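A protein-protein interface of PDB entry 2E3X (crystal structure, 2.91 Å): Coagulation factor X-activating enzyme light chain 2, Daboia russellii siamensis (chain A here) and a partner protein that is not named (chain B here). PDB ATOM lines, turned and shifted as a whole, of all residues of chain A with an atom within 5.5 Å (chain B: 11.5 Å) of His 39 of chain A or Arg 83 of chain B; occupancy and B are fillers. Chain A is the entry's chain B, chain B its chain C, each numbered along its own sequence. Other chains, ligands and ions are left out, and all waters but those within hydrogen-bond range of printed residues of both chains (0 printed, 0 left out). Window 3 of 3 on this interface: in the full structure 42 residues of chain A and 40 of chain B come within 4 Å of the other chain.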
ATOM      1  N   GLU A  28     -37.102 -10.849 -11.694  1.00  0.00           N
ATOM      2  CA  GLU A  28     -36.831 -11.032 -10.273  1.00  0.00           C
ATOM      3  C   GLU A  28     -37.908 -11.918  -9.654  1.00  0.00           C
ATOM      4  O   GLU A  28     -37.611 -12.892  -8.967  1.00  0.00           O
ATOM      5  CB  GLU A  28     -36.818  -9.682  -9.555  1.00  0.00           C
ATOM      6  CG  GLU A  28     -36.839  -9.800  -8.037  1.00  0.00           C
ATOM      7  CD  GLU A  28     -35.544 -10.349  -7.453  1.00  0.00           C
ATOM      8  OE1 GLU A  28     -34.737 -10.941  -8.205  1.00  0.00           O
ATOM      9  OE2 GLU A  28     -35.339 -10.194  -6.230  1.00  0.00           O
ATOM     10  N   CYS A  31     -37.342 -15.338 -10.648  1.00  0.00           N
ATOM     11  CA  CYS A  31     -36.118 -15.925 -10.120  1.00  0.00           C
ATOM     12  C   CYS A  31     -36.337 -16.546  -8.749  1.00  0.00           C
ATOM     13  O   CYS A  31     -35.627 -17.474  -8.364  1.00  0.00           O
ATOM     14  CB  CYS A  31     -35.010 -14.872 -10.018  1.00  0.00           C
ATOM     15  SG  CYS A  31     -34.162 -14.477 -11.580  1.00  0.00           S
ATOM     16  N   MET A  32     -37.322 -16.039  -8.017  1.00  0.00           N
ATOM     17  CA  MET A  32     -37.609 -16.544  -6.680  1.00  0.00           C
ATOM     18  C   MET A  32     -38.948 -17.274  -6.563  1.00  0.00           C
ATOM     19  O   MET A  32     -39.836 -16.844  -5.831  1.00  0.00           O
ATOM     20  CB  MET A  32     -37.537 -15.388  -5.675  1.00  0.00           C
ATOM     21  CG  MET A  32     -38.353 -14.161  -6.064  1.00  0.00           C
ATOM     22  SD  MET A  32     -37.932 -12.674  -5.108  1.00  0.00           S
ATOM     23  CE  MET A  32     -39.008 -12.850  -3.684  1.00  0.00           C
ATOM     24  N   ASN A  37     -35.578 -19.164  -3.413  1.00  0.00           N
ATOM     25  CA  ASN A  37     -34.600 -18.210  -2.894  1.00  0.00           C
ATOM     26  C   ASN A  37     -33.962 -17.391  -4.009  1.00  0.00           C
ATOM     27  O   ASN A  37     -33.455 -16.296  -3.770  1.00  0.00           O
ATOM     28  CB  ASN A  37     -33.499 -18.933  -2.105  1.00  0.00           C
ATOM     29  CG  ASN A  37     -33.981 -19.450  -0.758  1.00  0.00           C
ATOM     30  OD1 ASN A  37     -34.400 -18.676   0.102  1.00  0.00           O
ATOM     31  ND2 ASN A  37     -33.917 -20.765  -0.571  1.00  0.00           N
ATOM     32  N   GLY A  38     -33.998 -17.928  -5.223  1.00  0.00           N
ATOM     33  CA  GLY A  38     -33.407 -17.248  -6.357  1.00  0.00           C
ATOM     34  C   GLY A  38     -33.622 -15.748  -6.394  1.00  0.00           C
ATOM     35  O   GLY A  38     -34.526 -15.210  -5.757  1.00  0.00           O
ATOM     36  N   HIS A  39     -32.763 -15.079  -7.154  1.00  0.00           N
ATOM     37  CA  HIS A  39     -32.812 -13.635  -7.333  1.00  0.00           C
ATOM     38  C   HIS A  39     -32.088 -13.358  -8.637  1.00  0.00           C
ATOM     39  O   HIS A  39     -31.507 -14.267  -9.230  1.00  0.00           O
ATOM     40  CB  HIS A  39     -32.076 -12.922  -6.197  1.00  0.00           C
ATOM     41  CG  HIS A  39     -32.846 -12.849  -4.918  1.00  0.00           C
ATOM     42  ND1 HIS A  39     -33.941 -12.028  -4.754  1.00  0.00           N
ATOM     43  CD2 HIS A  39     -32.665 -13.475  -3.731  1.00  0.00           C
ATOM     44  CE1 HIS A  39     -34.399 -12.150  -3.521  1.00  0.00           C
ATOM     45  NE2 HIS A  39     -33.643 -13.022  -2.880  1.00  0.00           N
ATOM     46  N   LEU A  40     -32.129 -12.111  -9.091  1.00  0.00           N
ATOM     47  CA  LEU A  40     -31.429 -11.750 -10.314  1.00  0.00           C
ATOM     48  C   LEU A  40     -29.952 -11.619  -9.961  1.00  0.00           C
ATOM     49  O   LEU A  40     -29.603 -11.107  -8.897  1.00  0.00           O
ATOM     50  CB  LEU A  40     -31.959 -10.428 -10.876  1.00  0.00           C
ATOM     51  CG  LEU A  40     -33.285 -10.496 -11.637  1.00  0.00           C
ATOM     52  CD1 LEU A  40     -33.716  -9.100 -12.055  1.00  0.00           C
ATOM     53  CD2 LEU A  40     -33.121 -11.390 -12.855  1.00  0.00           C
ATOM     54  N   VAL A  41     -29.088 -12.086 -10.852  1.00  0.00           N
ATOM     55  CA  VAL A  41     -27.653 -12.036 -10.620  1.00  0.00           C
ATOM     56  C   VAL A  41     -27.143 -10.780  -9.971  1.00  0.00           C
ATOM     57  O   VAL A  41     -27.385  -9.672 -10.447  1.00  0.00           O
ATOM     58  CB  VAL A  41     -26.846 -12.185 -11.913  1.00  0.00           C
ATOM     59  CG1 VAL A  41     -26.403 -13.621 -12.088  1.00  0.00           C
ATOM     60  CG2 VAL A  41     -27.673 -11.704 -13.092  1.00  0.00           C
ATOM     61  N   VAL A 127     -30.679 -13.593 -15.959  1.00  0.00           N
ATOM     62  CA  VAL A 127     -29.949 -14.716 -15.397  1.00  0.00           C
ATOM     63  C   VAL A 127     -30.146 -14.754 -13.887  1.00  0.00           C
ATOM     64  O   VAL A 127     -29.738 -13.838 -13.180  1.00  0.00           O
ATOM     65  CB  VAL A 127     -28.437 -14.623 -15.739  1.00  0.00           C
ATOM     66  CG1 VAL A 127     -28.022 -13.180 -15.885  1.00  0.00           C
ATOM     67  CG2 VAL A 127     -27.611 -15.291 -14.659  1.00  0.00           C
ATOM     68  N   CYS A 128     -30.789 -15.812 -13.402  1.00  0.00           N
ATOM     69  CA  CYS A 128     -31.039 -15.966 -11.972  1.00  0.00           C
ATOM     70  C   CYS A 128     -29.832 -16.569 -11.270  1.00  0.00           C
ATOM     71  O   CYS A 128     -29.093 -17.349 -11.860  1.00  0.00           O
ATOM     72  CB  CYS A 128     -32.253 -16.869 -11.720  1.00  0.00           C
ATOM     73  SG  CYS A 128     -33.845 -16.304 -12.407  1.00  0.00           S
ATOM     74  N   LYS A 129     -29.647 -16.205 -10.007  1.00  0.00           N
ATOM     75  CA  LYS A 129     -28.538 -16.703  -9.190  1.00  0.00           C
ATOM     76  C   LYS A 129     -29.192 -17.530  -8.090  1.00  0.00           C
ATOM     77  O   LYS A 129     -29.461 -17.031  -6.996  1.00  0.00           O
ATOM     78  CB  LYS A 129     -27.777 -15.518  -8.591  1.00  0.00           C
ATOM     79  CG  LYS A 129     -26.500 -15.849  -7.856  1.00  0.00           C
ATOM     80  CD  LYS A 129     -25.852 -14.561  -7.368  1.00  0.00           C
ATOM     81  CE  LYS A 129     -24.650 -14.819  -6.478  1.00  0.00           C
ATOM     82  NZ  LYS A 129     -24.135 -13.551  -5.884  1.00  0.00           N
ATOM     83  N   VAL A 130     -29.452 -18.795  -8.393  1.00  0.00           N
ATOM     84  CA  VAL A 130     -30.128 -19.700  -7.470  1.00  0.00           C
ATOM     85  C   VAL A 130     -29.224 -20.546  -6.571  1.00  0.00           C
ATOM     86  O   VAL A 130     -28.001 -20.542  -6.716  1.00  0.00           O
ATOM     87  CB  VAL A 130     -31.038 -20.657  -8.256  1.00  0.00           C
ATOM     88  CG1 VAL A 130     -32.072 -19.870  -9.027  1.00  0.00           C
ATOM     89  CG2 VAL A 130     -30.195 -21.499  -9.210  1.00  0.00           C
ATOM     90  N   MET B  78     -27.877   2.404  -4.232  1.00  0.00           N
ATOM     91  CA  MET B  78     -28.334   1.143  -4.792  1.00  0.00           C
ATOM     92  C   MET B  78     -28.211  -0.029  -3.828  1.00  0.00           C
ATOM     93  O   MET B  78     -27.783   0.130  -2.687  1.00  0.00           O
ATOM     94  CB  MET B  78     -27.553   0.846  -6.068  1.00  0.00           C
ATOM     95  CG  MET B  78     -27.596   1.971  -7.079  1.00  0.00           C
ATOM     96  SD  MET B  78     -26.606   1.615  -8.531  1.00  0.00           S
ATOM     97  CE  MET B  78     -24.963   2.122  -7.955  1.00  0.00           C
ATOM     98  N   GLU B  79     -28.591  -1.207  -4.308  1.00  0.00           N
ATOM     99  CA  GLU B  79     -28.542  -2.439  -3.532  1.00  0.00           C
ATOM    100  C   GLU B  79     -29.037  -3.535  -4.471  1.00  0.00           C
ATOM    101  O   GLU B  79     -29.817  -3.256  -5.380  1.00  0.00           O
ATOM    102  CB  GLU B  79     -29.467  -2.328  -2.317  1.00  0.00           C
ATOM    103  CG  GLU B  79     -29.341  -3.466  -1.313  1.00  0.00           C
ATOM    104  CD  GLU B  79     -30.423  -3.426  -0.244  1.00  0.00           C
ATOM    105  OE1 GLU B  79     -31.609  -3.608  -0.595  1.00  0.00           O
ATOM    106  OE2 GLU B  79     -30.091  -3.212   0.943  1.00  0.00           O
ATOM    107  N   TRP B  80     -28.588  -4.769  -4.277  1.00  0.00           N
ATOM    108  CA  TRP B  80     -29.043  -5.850  -5.146  1.00  0.00           C
ATOM    109  C   TRP B  80     -30.377  -6.383  -4.634  1.00  0.00           C
ATOM    110  O   TRP B  80     -30.703  -6.225  -3.458  1.00  0.00           O
ATOM    111  CB  TRP B  80     -27.997  -6.969  -5.214  1.00  0.00           C
ATOM    112  CG  TRP B  80     -26.644  -6.480  -5.682  1.00  0.00           C
ATOM    113  CD1 TRP B  80     -25.622  -6.022  -4.900  1.00  0.00           C
ATOM    114  CD2 TRP B  80     -26.201  -6.334  -7.041  1.00  0.00           C
ATOM    115  NE1 TRP B  80     -24.576  -5.595  -5.681  1.00  0.00           N
ATOM    116  CE2 TRP B  80     -24.903  -5.773  -6.999  1.00  0.00           C
ATOM    117  CE3 TRP B  80     -26.776  -6.613  -8.288  1.00  0.00           C
ATOM    118  CZ2 TRP B  80     -24.170  -5.489  -8.158  1.00  0.00           C
ATOM    119  CZ3 TRP B  80     -26.046  -6.330  -9.439  1.00  0.00           C
ATOM    120  CH2 TRP B  80     -24.755  -5.771  -9.363  1.00  0.00           C
ATOM    121  N   SER B  81     -31.157  -6.996  -5.519  1.00  0.00           N
ATOM    122  CA  SER B  81     -32.459  -7.524  -5.125  1.00  0.00           C
ATOM    123  C   SER B  81     -32.337  -8.629  -4.076  1.00  0.00           C
ATOM    124  O   SER B  81     -33.307  -8.936  -3.383  1.00  0.00           O
ATOM    125  CB  SER B  81     -33.224  -8.045  -6.347  1.00  0.00           C
ATOM    126  OG  SER B  81     -32.546  -9.123  -6.967  1.00  0.00           O
ATOM    127  N   ASP B  82     -31.150  -9.225  -3.962  1.00  0.00           N
ATOM    128  CA  ASP B  82     -30.920 -10.278  -2.976  1.00  0.00           C
ATOM    129  C   ASP B  82     -30.447  -9.665  -1.660  1.00  0.00           C
ATOM    130  O   ASP B  82     -29.773 -10.313  -0.867  1.00  0.00           O
ATOM    131  CB  ASP B  82     -29.881 -11.287  -3.476  1.00  0.00           C
ATOM    132  CG  ASP B  82     -28.522 -10.657  -3.734  1.00  0.00           C
ATOM    133  OD1 ASP B  82     -28.136  -9.726  -2.994  1.00  0.00           O
ATOM    134  OD2 ASP B  82     -27.831 -11.106  -4.675  1.00  0.00           O
ATOM    135  N   ARG B  83     -30.802  -8.403  -1.449  1.00  0.00           N
ATOM    136  CA  ARG B  83     -30.451  -7.668  -0.237  1.00  0.00           C
ATOM    137  C   ARG B  83     -28.959  -7.510   0.022  1.00  0.00           C
ATOM    138  O   ARG B  83     -28.560  -6.947   1.041  1.00  0.00           O
ATOM    139  CB  ARG B  83     -31.142  -8.307   0.970  1.00  0.00           C
ATOM    140  CG  ARG B  83     -32.645  -8.052   0.980  1.00  0.00           C
ATOM    141  CD  ARG B  83     -33.374  -8.870   2.028  1.00  0.00           C
ATOM    142  NE  ARG B  83     -33.323 -10.302   1.741  1.00  0.00           N
ATOM    143  CZ  ARG B  83     -33.816 -10.868   0.642  1.00  0.00           C
ATOM    144  NH1 ARG B  83     -34.403 -10.125  -0.286  1.00  0.00           N
ATOM    145  NH2 ARG B  83     -33.722 -12.182   0.474  1.00  0.00           N
ATOM    146  N   GLY B  84     -28.136  -7.987  -0.906  1.00  0.00           N
ATOM    147  CA  GLY B  84     -26.700  -7.857  -0.741  1.00  0.00           C
ATOM    148  C   GLY B  84     -26.278  -6.408  -0.895  1.00  0.00           C
ATOM    149  O   GLY B  84     -27.000  -5.619  -1.502  1.00  0.00           O
ATOM    150  N   ASN B  85     -25.119  -6.050  -0.351  1.00  0.00           N
ATOM    151  CA  ASN B  85     -24.624  -4.677  -0.444  1.00  0.00           C
ATOM    152  C   ASN B  85     -23.908  -4.463  -1.770  1.00  0.00           C
ATOM    153  O   ASN B  85     -23.416  -5.416  -2.371  1.00  0.00           O
ATOM    154  CB  ASN B  85     -23.661  -4.382   0.704  1.00  0.00           C
ATOM    155  CG  ASN B  85     -24.138  -4.955   2.017  1.00  0.00           C
ATOM    156  OD1 ASN B  85     -25.295  -4.774   2.397  1.00  0.00           O
ATOM    157  ND2 ASN B  85     -23.249  -5.649   2.724  1.00  0.00           N
ATOM    158  N   VAL B  86     -23.848  -3.215  -2.224  1.00  0.00           N
ATOM    159  CA  VAL B  86     -23.183  -2.899  -3.481  1.00  0.00           C
ATOM    160  C   VAL B  86     -21.833  -2.218  -3.261  1.00  0.00           C
ATOM    161  O   VAL B  86     -21.748  -0.993  -3.120  1.00  0.00           O
ATOM    162  CB  VAL B  86     -24.060  -1.979  -4.379  1.00  0.00           C
ATOM    163  CG1 VAL B  86     -23.321  -1.643  -5.670  1.00  0.00           C
ATOM    164  CG2 VAL B  86     -25.372  -2.660  -4.702  1.00  0.00           C
ATOM    165  N   LYS B  87     -20.777  -3.022  -3.223  1.00  0.00           N
ATOM    166  CA  LYS B  87     -19.428  -2.505  -3.054  1.00  0.00           C
ATOM    167  C   LYS B  87     -18.850  -2.333  -4.454  1.00  0.00           C
ATOM    168  O   LYS B  87     -18.374  -1.259  -4.823  1.00  0.00           O
ATOM    169  CB  LYS B  87     -18.573  -3.497  -2.267  1.00  0.00           C
ATOM    170  CG  LYS B  87     -17.126  -3.059  -2.074  1.00  0.00           C
ATOM    171  CD  LYS B  87     -16.323  -4.120  -1.329  1.00  0.00           C
ATOM    172  CE  LYS B  87     -14.888  -3.670  -1.082  1.00  0.00           C
ATOM    173  NZ  LYS B  87     -14.098  -4.702  -0.349  1.00  0.00           N
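OG of Ser 81 of chain B sits close to OE2 of Glu 28 of chain A (3.1 Å). A ring nitrogen (ND1) of His 39 of chain A sits close to the backbone carbonyl oxygen (O) of Ser 81 of chain B, 3.4 Å away. A ring nitrogen (NE2) of His 39 of chain A is in hydrogen-bond range of the guanidinium group (NH2) of Arg 83 of chain B (3.5 Å).
The side-chain carboxylate (OE2) of Glu 28 of chain A sits at hydrogen-bond distance from a ring nitrogen (ND1) of His 39 of chain A, at 2.7 Å. The side-chain carboxylate (OE1) of Glu 28 of chain A is in hydrogen-bond range of the backbone NH (N) of Leu 40 of chain A (3.0 Å). A ring nitrogen (NE2) of His 39 of chain A lies close to the backbone carbonyl oxygen of Asn 37 of chain A (3.4 Å). N of Val 41 of chain A lies close to O of Val 127 of chain A (3.0 Å). The backbone carbonyl oxygen of Ser 81 of chain B lies within hydrogen-bond range of the guanidinium group of Arg 83 of chain B (3.5 Å). The side-chain sulfur of Cys 31 of chain A forms a disulfide with the side-chain sulfur of Cys 128 of chain A (2.0 Å).
Among the printed residues, merely in contact across the chains: His 39 of chain A with Asp 82 of chain B (3.6 Å), Leu 40 of chain A with Ser 81 of chain B (3.7 Å) and Val 41 of chain A with Trp 80 of chain B (3.7 Å).
Of the printed residues of chain B, His 39 of chain A touches Ser 81 (3.4 Å), Asp 82 (3.6 Å) and Arg 83 (3.5 Å). Glu 28 of chain A touches one residue of chain B. No residue of chain B comes within 4 Å of Cys 31 of chain A. No residue of chain B comes within 4 Å of Gly 38 of chain A. Printed residues of chain B within 4 Å of Leu 40 of chain A: Ser 81 (3.7 Å). Val 41 of chain A touches just one residue of chain B: Trp 80 (3.7 Å). No residue of chain B comes within 4 Å of Val 130 of chain A. Of the printed residues of chain A, Asp 82 of chain B touches His 39. Printed residues of chain A within 4 Å of Ser 81 of chain B: Glu 28 (3.0 Å), His 39 (3.4 Å) and Leu 40 (3.7 Å). Printed residues of chain A within 4 Å of Trp 80 of chain B: Val 41. Val 127 of chain A touches none of the printed residues of chain B. The nearest residue of chain B that does not touch His 39 of chain A is Trp 80 of chain B (6.7 Å). The nearest printed residue of chain A that does not touch Ser 81 of chain B is Val 41 of chain A (6.0 Å).
Printed residues of chain A that touch a printed residue of chain B: Glu 28, His 39, Leu 40 and Val 41. Hydrophobic or aromatic side chains of chain A within 4 Å of the printed part of chain B: His 39. Among the printed residues, no Asp or Glu carboxylate lies within 4 Å of a Lys or Arg side-chain nitrogen of the other chain.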
